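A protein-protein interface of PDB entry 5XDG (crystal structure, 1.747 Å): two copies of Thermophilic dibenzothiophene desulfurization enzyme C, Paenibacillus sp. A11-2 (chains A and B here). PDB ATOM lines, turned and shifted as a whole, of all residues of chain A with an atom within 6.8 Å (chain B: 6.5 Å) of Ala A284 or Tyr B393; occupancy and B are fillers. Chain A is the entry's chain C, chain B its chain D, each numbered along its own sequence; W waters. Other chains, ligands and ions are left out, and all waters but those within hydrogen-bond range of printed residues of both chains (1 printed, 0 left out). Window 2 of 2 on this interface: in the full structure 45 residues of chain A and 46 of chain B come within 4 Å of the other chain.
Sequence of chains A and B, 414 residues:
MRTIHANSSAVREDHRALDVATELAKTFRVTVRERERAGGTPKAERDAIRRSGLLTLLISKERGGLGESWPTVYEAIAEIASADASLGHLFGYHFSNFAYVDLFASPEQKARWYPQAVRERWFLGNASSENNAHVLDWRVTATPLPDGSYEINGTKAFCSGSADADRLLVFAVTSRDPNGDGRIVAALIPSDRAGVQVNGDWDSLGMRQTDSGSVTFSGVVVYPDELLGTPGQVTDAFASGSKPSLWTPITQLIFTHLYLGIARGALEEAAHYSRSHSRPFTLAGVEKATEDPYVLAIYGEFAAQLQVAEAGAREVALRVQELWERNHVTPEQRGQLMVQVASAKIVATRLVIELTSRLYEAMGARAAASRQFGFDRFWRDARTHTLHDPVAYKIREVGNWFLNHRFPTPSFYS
The side-chain hydroxyl of Tyr B393 sits at hydrogen-bond distance from the side-chain carboxylate of Asp A292.
The backbone NH (N) of Val A295 sits at hydrogen-bond distance from the side-chain carboxylate (OD1) of Asp A292, at 3.0 Å.
O of Phe A281 is in hydrogen-bond range of N of Val A286.
OD1 of Asp A292 is in hydrogen-bond range of N of Tyr A294 (2.8 Å).
Phe A281 touches Pro B390.
Tyr B393 touches Phe A281.
Leu B136 touches Thr A282.
Leu B136 touches Leu A283.
Ala A284 touches Tyr B393.
Tyr B393 touches Val A286.
Tyr A294 touches Ala B392.
CD2 of Tyr A294 touches CZ of Tyr B393, 3.7 Å away.
OH of Tyr A294 touches CG of Arg B396, at 3.7 Å.
Printed residues of chain B within 4 Å of Phe A281: Pro B390 and Tyr B393.
Ala A284 touches just one residue of chain B: Tyr B393.
Printed residues of chain B within 4 Å of Asp A292: Tyr B393.
Of the printed residues of chain A, Leu B136 touches Thr A282 and Leu A283.
Val B391 touches none of the printed residues of chain A.
Of the printed residues of chain A, Ala B392 touches Tyr A294.
Of the printed residues of chain A, Tyr B393 touches Phe A281, Ala A284, Val A286, Asp A292 and Tyr A294.
Of the printed residues of chain A, Arg B396 touches Tyr A294 (3.7 Å).
Glu B397 touches none of the printed residues of chain A.
The nearest printed residue of chain A that does not touch Tyr B393 is Pro A293 (4.01 Å).
The nearest printed residue of chain B that does not touch Tyr A294 is Ile B395 (6.3 Å).
Printed residues of chain B that touch a printed residue of chain A: Leu B136, Pro B390, Ala B392, Tyr B393 and Arg B396.
Hydrophobic or aromatic side chains of chain A within 4 Å of the printed part of chain B: Phe A281, Leu A283, Ala A284, Val A286 and Tyr A294.
Among the printed residues, 10 pairs touch across the chains.
Among the printed residues, no Asp or Glu carboxylate lies within 4 Å of a Lys or Arg side-chain nitrogen of the other chain.
No position is printed for both chains.
Of the 10 pairs that touch across the chains among the printed residues, none has its exchanged pair printed and touching as well.
Water W1 lies within hydrogen-bond range of the backbone carbonyl oxygen of Ala A284 (3.2 Å) and the guanidinium group of Arg B396 (3.4 Å).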
ATOM      1  N   PHE A 281     -12.755  17.751 -25.254  1.00  0.00           N
ATOM      2  CA  PHE A 281     -13.003  18.143 -23.864  1.00  0.00           C
ATOM      3  C   PHE A 281     -14.479  17.900 -23.559  1.00  0.00           C
ATOM      4  O   PHE A 281     -15.318  18.804 -23.557  1.00  0.00           O
ATOM      5  CB  PHE A 281     -12.603  19.592 -23.608  1.00  0.00           C
ATOM      6  CG  PHE A 281     -12.466  19.928 -22.136  1.00  0.00           C
ATOM      7  CD1 PHE A 281     -11.603  19.203 -21.328  1.00  0.00           C
ATOM      8  CD2 PHE A 281     -13.190  20.969 -21.566  1.00  0.00           C
ATOM      9  CE1 PHE A 281     -11.471  19.493 -19.979  1.00  0.00           C
ATOM     10  CE2 PHE A 281     -13.060  21.271 -20.206  1.00  0.00           C
ATOM     11  CZ  PHE A 281     -12.199  20.531 -19.415  1.00  0.00           C
ATOM     12  N   THR A 282     -14.790  16.630 -23.306  1.00  0.00           N
ATOM     13  CA  THR A 282     -16.166  16.196 -23.100  1.00  0.00           C
ATOM     14  C   THR A 282     -16.800  16.812 -21.865  1.00  0.00           C
ATOM     15  O   THR A 282     -18.034  16.855 -21.778  1.00  0.00           O
ATOM     16  CB  THR A 282     -16.209  14.674 -23.003  1.00  0.00           C
ATOM     17  OG1 THR A 282     -15.432  14.253 -21.876  1.00  0.00           O
ATOM     18  CG2 THR A 282     -15.616  14.052 -24.271  1.00  0.00           C
ATOM     19  N   LEU A 283     -16.002  17.298 -20.910  1.00  0.00           N
ATOM     20  CA  LEU A 283     -16.591  18.013 -19.785  1.00  0.00           C
ATOM     21  C   LEU A 283     -17.442  19.176 -20.253  1.00  0.00           C
ATOM     22  O   LEU A 283     -18.412  19.546 -19.582  1.00  0.00           O
ATOM     23  CB  LEU A 283     -15.506  18.509 -18.830  1.00  0.00           C
ATOM     24  CG  LEU A 283     -15.553  17.654 -17.567  1.00  0.00           C
ATOM     25  CD1 LEU A 283     -14.184  17.095 -17.270  1.00  0.00           C
ATOM     26  CD2 LEU A 283     -16.110  18.439 -16.390  1.00  0.00           C
ATOM     27  N   ALA A 284     -17.112  19.758 -21.409  1.00  0.00           N
ATOM     28  CA  ALA A 284     -17.903  20.848 -21.963  1.00  0.00           C
ATOM     29  C   ALA A 284     -18.777  20.397 -23.130  1.00  0.00           C
ATOM     30  O   ALA A 284     -19.296  21.238 -23.873  1.00  0.00           O
ATOM     31  CB  ALA A 284     -16.995  22.005 -22.385  1.00  0.00           C
ATOM     32  N   GLY A 285     -18.951  19.089 -23.308  1.00  0.00           N
ATOM     33  CA  GLY A 285     -19.823  18.597 -24.352  1.00  0.00           C
ATOM     34  C   GLY A 285     -19.239  18.598 -25.741  1.00  0.00           C
ATOM     35  O   GLY A 285     -19.996  18.548 -26.714  1.00  0.00           O
ATOM     36  N   VAL A 286     -17.920  18.675 -25.872  1.00  0.00           N
ATOM     37  CA  VAL A 286     -17.271  18.601 -27.175  1.00  0.00           C
ATOM     38  C   VAL A 286     -17.148  17.135 -27.580  1.00  0.00           C
ATOM     39  O   VAL A 286     -16.701  16.295 -26.789  1.00  0.00           O
ATOM     40  CB  VAL A 286     -15.893  19.286 -27.133  1.00  0.00           C
ATOM     41  CG1 VAL A 286     -15.095  18.976 -28.395  1.00  0.00           C
ATOM     42  CG2 VAL A 286     -16.041  20.784 -26.934  1.00  0.00           C
ATOM     43  N   ASP A 292     -13.812  21.740 -31.751  1.00  0.00           N
ATOM     44  CA  ASP A 292     -13.781  22.601 -30.576  1.00  0.00           C
ATOM     45  C   ASP A 292     -13.656  24.062 -31.008  1.00  0.00           C
ATOM     46  O   ASP A 292     -12.769  24.387 -31.807  1.00  0.00           O
ATOM     47  CB  ASP A 292     -12.604  22.216 -29.684  1.00  0.00           C
ATOM     48  CG  ASP A 292     -12.556  23.018 -28.394  1.00  0.00           C
ATOM     49  OD1 ASP A 292     -12.245  24.228 -28.440  1.00  0.00           O
ATOM     50  OD2 ASP A 292     -12.815  22.424 -27.334  1.00  0.00           O
ATOM     51  N   PRO A 293     -14.503  24.965 -30.500  1.00  0.00           N
ATOM     52  CA  PRO A 293     -14.463  26.356 -30.993  1.00  0.00           C
ATOM     53  C   PRO A 293     -13.161  27.066 -30.675  1.00  0.00           C
ATOM     54  O   PRO A 293     -12.744  27.957 -31.425  1.00  0.00           O
ATOM     55  CB  PRO A 293     -15.645  27.024 -30.273  1.00  0.00           C
ATOM     56  CG  PRO A 293     -15.907  26.136 -29.075  1.00  0.00           C
ATOM     57  CD  PRO A 293     -15.588  24.752 -29.525  1.00  0.00           C
ATOM     58  N   TYR A 294     -12.528  26.726 -29.561  1.00  0.00           N
ATOM     59  CA  TYR A 294     -11.298  27.400 -29.182  1.00  0.00           C
ATOM     60  C   TYR A 294     -10.083  26.787 -29.879  1.00  0.00           C
ATOM     61  O   TYR A 294      -9.132  27.508 -30.204  1.00  0.00           O
ATOM     62  CB  TYR A 294     -11.181  27.377 -27.652  1.00  0.00           C
ATOM     63  CG  TYR A 294     -12.428  27.956 -26.985  1.00  0.00           C
ATOM     64  CD1 TYR A 294     -12.909  29.217 -27.332  1.00  0.00           C
ATOM     65  CD2 TYR A 294     -13.151  27.213 -26.059  1.00  0.00           C
ATOM     66  CE1 TYR A 294     -14.067  29.734 -26.756  1.00  0.00           C
ATOM     67  CE2 TYR A 294     -14.306  27.723 -25.468  1.00  0.00           C
ATOM     68  CZ  TYR A 294     -14.754  28.979 -25.817  1.00  0.00           C
ATOM     69  OH  TYR A 294     -15.893  29.475 -25.224  1.00  0.00           O
ATOM     70  N   VAL A 295     -10.105  25.484 -30.159  1.00  0.00           N
ATOM     71  CA  VAL A 295      -9.076  24.910 -31.026  1.00  0.00           C
ATOM     72  C   VAL A 295      -9.130  25.568 -32.405  1.00  0.00           C
ATOM     73  O   VAL A 295      -8.103  25.995 -32.956  1.00  0.00           O
ATOM     74  CB  VAL A 295      -9.231  23.381 -31.119  1.00  0.00           C
ATOM     75  CG1 VAL A 295      -8.256  22.812 -32.152  1.00  0.00           C
ATOM     76  CG2 VAL A 295      -8.990  22.739 -29.753  1.00  0.00           C
ATOM     77  N   LEU B 136     -12.990  12.066 -19.180  1.00  0.00           N
ATOM     78  CA  LEU B 136     -14.033  11.466 -18.350  1.00  0.00           C
ATOM     79  C   LEU B 136     -14.066   9.942 -18.419  1.00  0.00           C
ATOM     80  O   LEU B 136     -14.708   9.314 -17.569  1.00  0.00           O
ATOM     81  CB  LEU B 136     -15.407  12.009 -18.748  1.00  0.00           C
ATOM     82  CG  LEU B 136     -15.614  13.512 -18.583  1.00  0.00           C
ATOM     83  CD1 LEU B 136     -17.067  13.874 -18.819  1.00  0.00           C
ATOM     84  CD2 LEU B 136     -15.157  13.966 -17.201  1.00  0.00           C
ATOM     85  N   PRO B 390      -7.585  22.762 -20.031  1.00  0.00           N
ATOM     86  CA  PRO B 390      -7.500  23.849 -21.023  1.00  0.00           C
ATOM     87  C   PRO B 390      -7.928  25.199 -20.457  1.00  0.00           C
ATOM     88  O   PRO B 390      -9.062  25.369 -20.003  1.00  0.00           O
ATOM     89  CB  PRO B 390      -8.435  23.379 -22.146  1.00  0.00           C
ATOM     90  CG  PRO B 390      -9.311  22.336 -21.520  1.00  0.00           C
ATOM     91  CD  PRO B 390      -8.521  21.701 -20.442  1.00  0.00           C
ATOM     92  N   VAL B 391      -7.018  26.175 -20.516  1.00  0.00           N
ATOM     93  CA  VAL B 391      -7.324  27.510 -20.023  1.00  0.00           C
ATOM     94  C   VAL B 391      -8.508  28.108 -20.772  1.00  0.00           C
ATOM     95  O   VAL B 391      -9.222  28.963 -20.232  1.00  0.00           O
ATOM     96  CB  VAL B 391      -6.076  28.416 -20.102  1.00  0.00           C
ATOM     97  CG1 VAL B 391      -5.733  28.779 -21.545  1.00  0.00           C
ATOM     98  CG2 VAL B 391      -6.284  29.675 -19.249  1.00  0.00           C
ATOM     99  N   ALA B 392      -8.756  27.651 -22.001  1.00  0.00           N
ATOM    100  CA  ALA B 392      -9.898  28.151 -22.760  1.00  0.00           C
ATOM    101  C   ALA B 392     -11.207  27.915 -22.019  1.00  0.00           C
ATOM    102  O   ALA B 392     -12.130  28.729 -22.114  1.00  0.00           O
ATOM    103  CB  ALA B 392      -9.943  27.493 -24.138  1.00  0.00           C
ATOM    104  N   TYR B 393     -11.316  26.795 -21.290  1.00  0.00           N
ATOM    105  CA  TYR B 393     -12.556  26.507 -20.579  1.00  0.00           C
ATOM    106  C   TYR B 393     -12.585  27.113 -19.183  1.00  0.00           C
ATOM    107  O   TYR B 393     -13.679  27.380 -18.669  1.00  0.00           O
ATOM    108  CB  TYR B 393     -12.819  24.988 -20.556  1.00  0.00           C
ATOM    109  CG  TYR B 393     -13.301  24.586 -21.930  1.00  0.00           C
ATOM    110  CD1 TYR B 393     -14.615  24.844 -22.324  1.00  0.00           C
ATOM    111  CD2 TYR B 393     -12.427  24.061 -22.871  1.00  0.00           C
ATOM    112  CE1 TYR B 393     -15.057  24.538 -23.611  1.00  0.00           C
ATOM    113  CE2 TYR B 393     -12.861  23.763 -24.164  1.00  0.00           C
ATOM    114  CZ  TYR B 393     -14.175  24.004 -24.516  1.00  0.00           C
ATOM    115  OH  TYR B 393     -14.608  23.694 -25.783  1.00  0.00           O
ATOM    116  N   LYS B 394     -11.427  27.416 -18.592  1.00  0.00           N
ATOM    117  CA  LYS B 394     -11.426  28.322 -17.446  1.00  0.00           C
ATOM    118  C   LYS B 394     -11.947  29.698 -17.847  1.00  0.00           C
ATOM    119  O   LYS B 394     -12.747  30.309 -17.128  1.00  0.00           O
ATOM    120  CB  LYS B 394     -10.020  28.422 -16.856  1.00  0.00           C
ATOM    121  CG  LYS B 394      -9.562  27.162 -16.179  1.00  0.00           C
ATOM    122  CD  LYS B 394     -10.236  27.006 -14.819  1.00  0.00           C
ATOM    123  CE  LYS B 394     -10.319  25.551 -14.409  1.00  0.00           C
ATOM    124  NZ  LYS B 394     -11.360  24.819 -15.189  1.00  0.00           N
ATOM    125  N   ILE B 395     -11.526  30.194 -19.012  1.00  0.00           N
ATOM    126  CA  ILE B 395     -12.048  31.467 -19.512  1.00  0.00           C
ATOM    127  C   ILE B 395     -13.556  31.375 -19.747  1.00  0.00           C
ATOM    128  O   ILE B 395     -14.317  32.274 -19.365  1.00  0.00           O
ATOM    129  CB  ILE B 395     -11.290  31.893 -20.787  1.00  0.00           C
ATOM    130  CG1 ILE B 395      -9.849  32.287 -20.438  1.00  0.00           C
ATOM    131  CG2 ILE B 395     -12.014  33.046 -21.486  1.00  0.00           C
ATOM    132  CD1 ILE B 395      -8.923  32.451 -21.640  1.00  0.00           C
ATOM    133  N   ARG B 396     -14.020  30.290 -20.379  1.00  0.00           N
ATOM    134  CA  ARG B 396     -15.459  30.153 -20.592  1.00  0.00           C
ATOM    135  C   ARG B 396     -16.198  30.131 -19.259  1.00  0.00           C
ATOM    136  O   ARG B 396     -17.269  30.733 -19.120  1.00  0.00           O
ATOM    137  CB  ARG B 396     -15.779  28.894 -21.402  1.00  0.00           C
ATOM    138  CG  ARG B 396     -17.273  28.797 -21.847  1.00  0.00           C
ATOM    139  CD  ARG B 396     -17.603  27.451 -22.472  1.00  0.00           C
ATOM    140  NE  ARG B 396     -18.928  27.422 -23.103  1.00  0.00           N
ATOM    141  CZ  ARG B 396     -20.071  27.284 -22.431  1.00  0.00           C
ATOM    142  NH1 ARG B 396     -20.060  27.167 -21.108  1.00  0.00           N
ATOM    143  NH2 ARG B 396     -21.232  27.266 -23.079  1.00  0.00           N
ATOM    144  N   GLU B 397     -15.636  29.438 -18.269  1.00  0.00           N
ATOM    145  CA  GLU B 397     -16.292  29.349 -16.966  1.00  0.00           C
ATOM    146  C   GLU B 397     -16.440  30.721 -16.318  1.00  0.00           C
ATOM    147  O   GLU B 397     -17.505  31.044 -15.776  1.00  0.00           O
ATOM    148  CB  GLU B 397     -15.525  28.376 -16.069  1.00  0.00           C
ATOM    149  CG  GLU B 397     -15.767  26.914 -16.475  1.00  0.00           C
ATOM    150  CD  GLU B 397     -14.611  25.974 -16.148  1.00  0.00           C
ATOM    151  OE1 GLU B 397     -13.717  26.345 -15.352  1.00  0.00           O
ATOM    152  OE2 GLU B 397     -14.598  24.855 -16.707  1.00  0.00           O
ATOM    153  N   VAL B 398     -15.403  31.562 -16.387  1.00  0.00           N
ATOM    154  CA  VAL B 398     -15.522  32.898 -15.810  1.00  0.00           C
ATOM    155  C   VAL B 398     -16.512  33.730 -16.611  1.00  0.00           C
ATOM    156  O   VAL B 398     -17.297  34.494 -16.040  1.00  0.00           O
ATOM    157  CB  VAL B 398     -14.142  33.578 -15.708  1.00  0.00           C
ATOM    158  CG1 VAL B 398     -14.284  35.042 -15.251  1.00  0.00           C
ATOM    159  CG2 VAL B 398     -13.250  32.800 -14.761  1.00  0.00           C
HETATM  160  O   HOH W   1     -19.191  24.378 -24.649  1.00  0.00           O
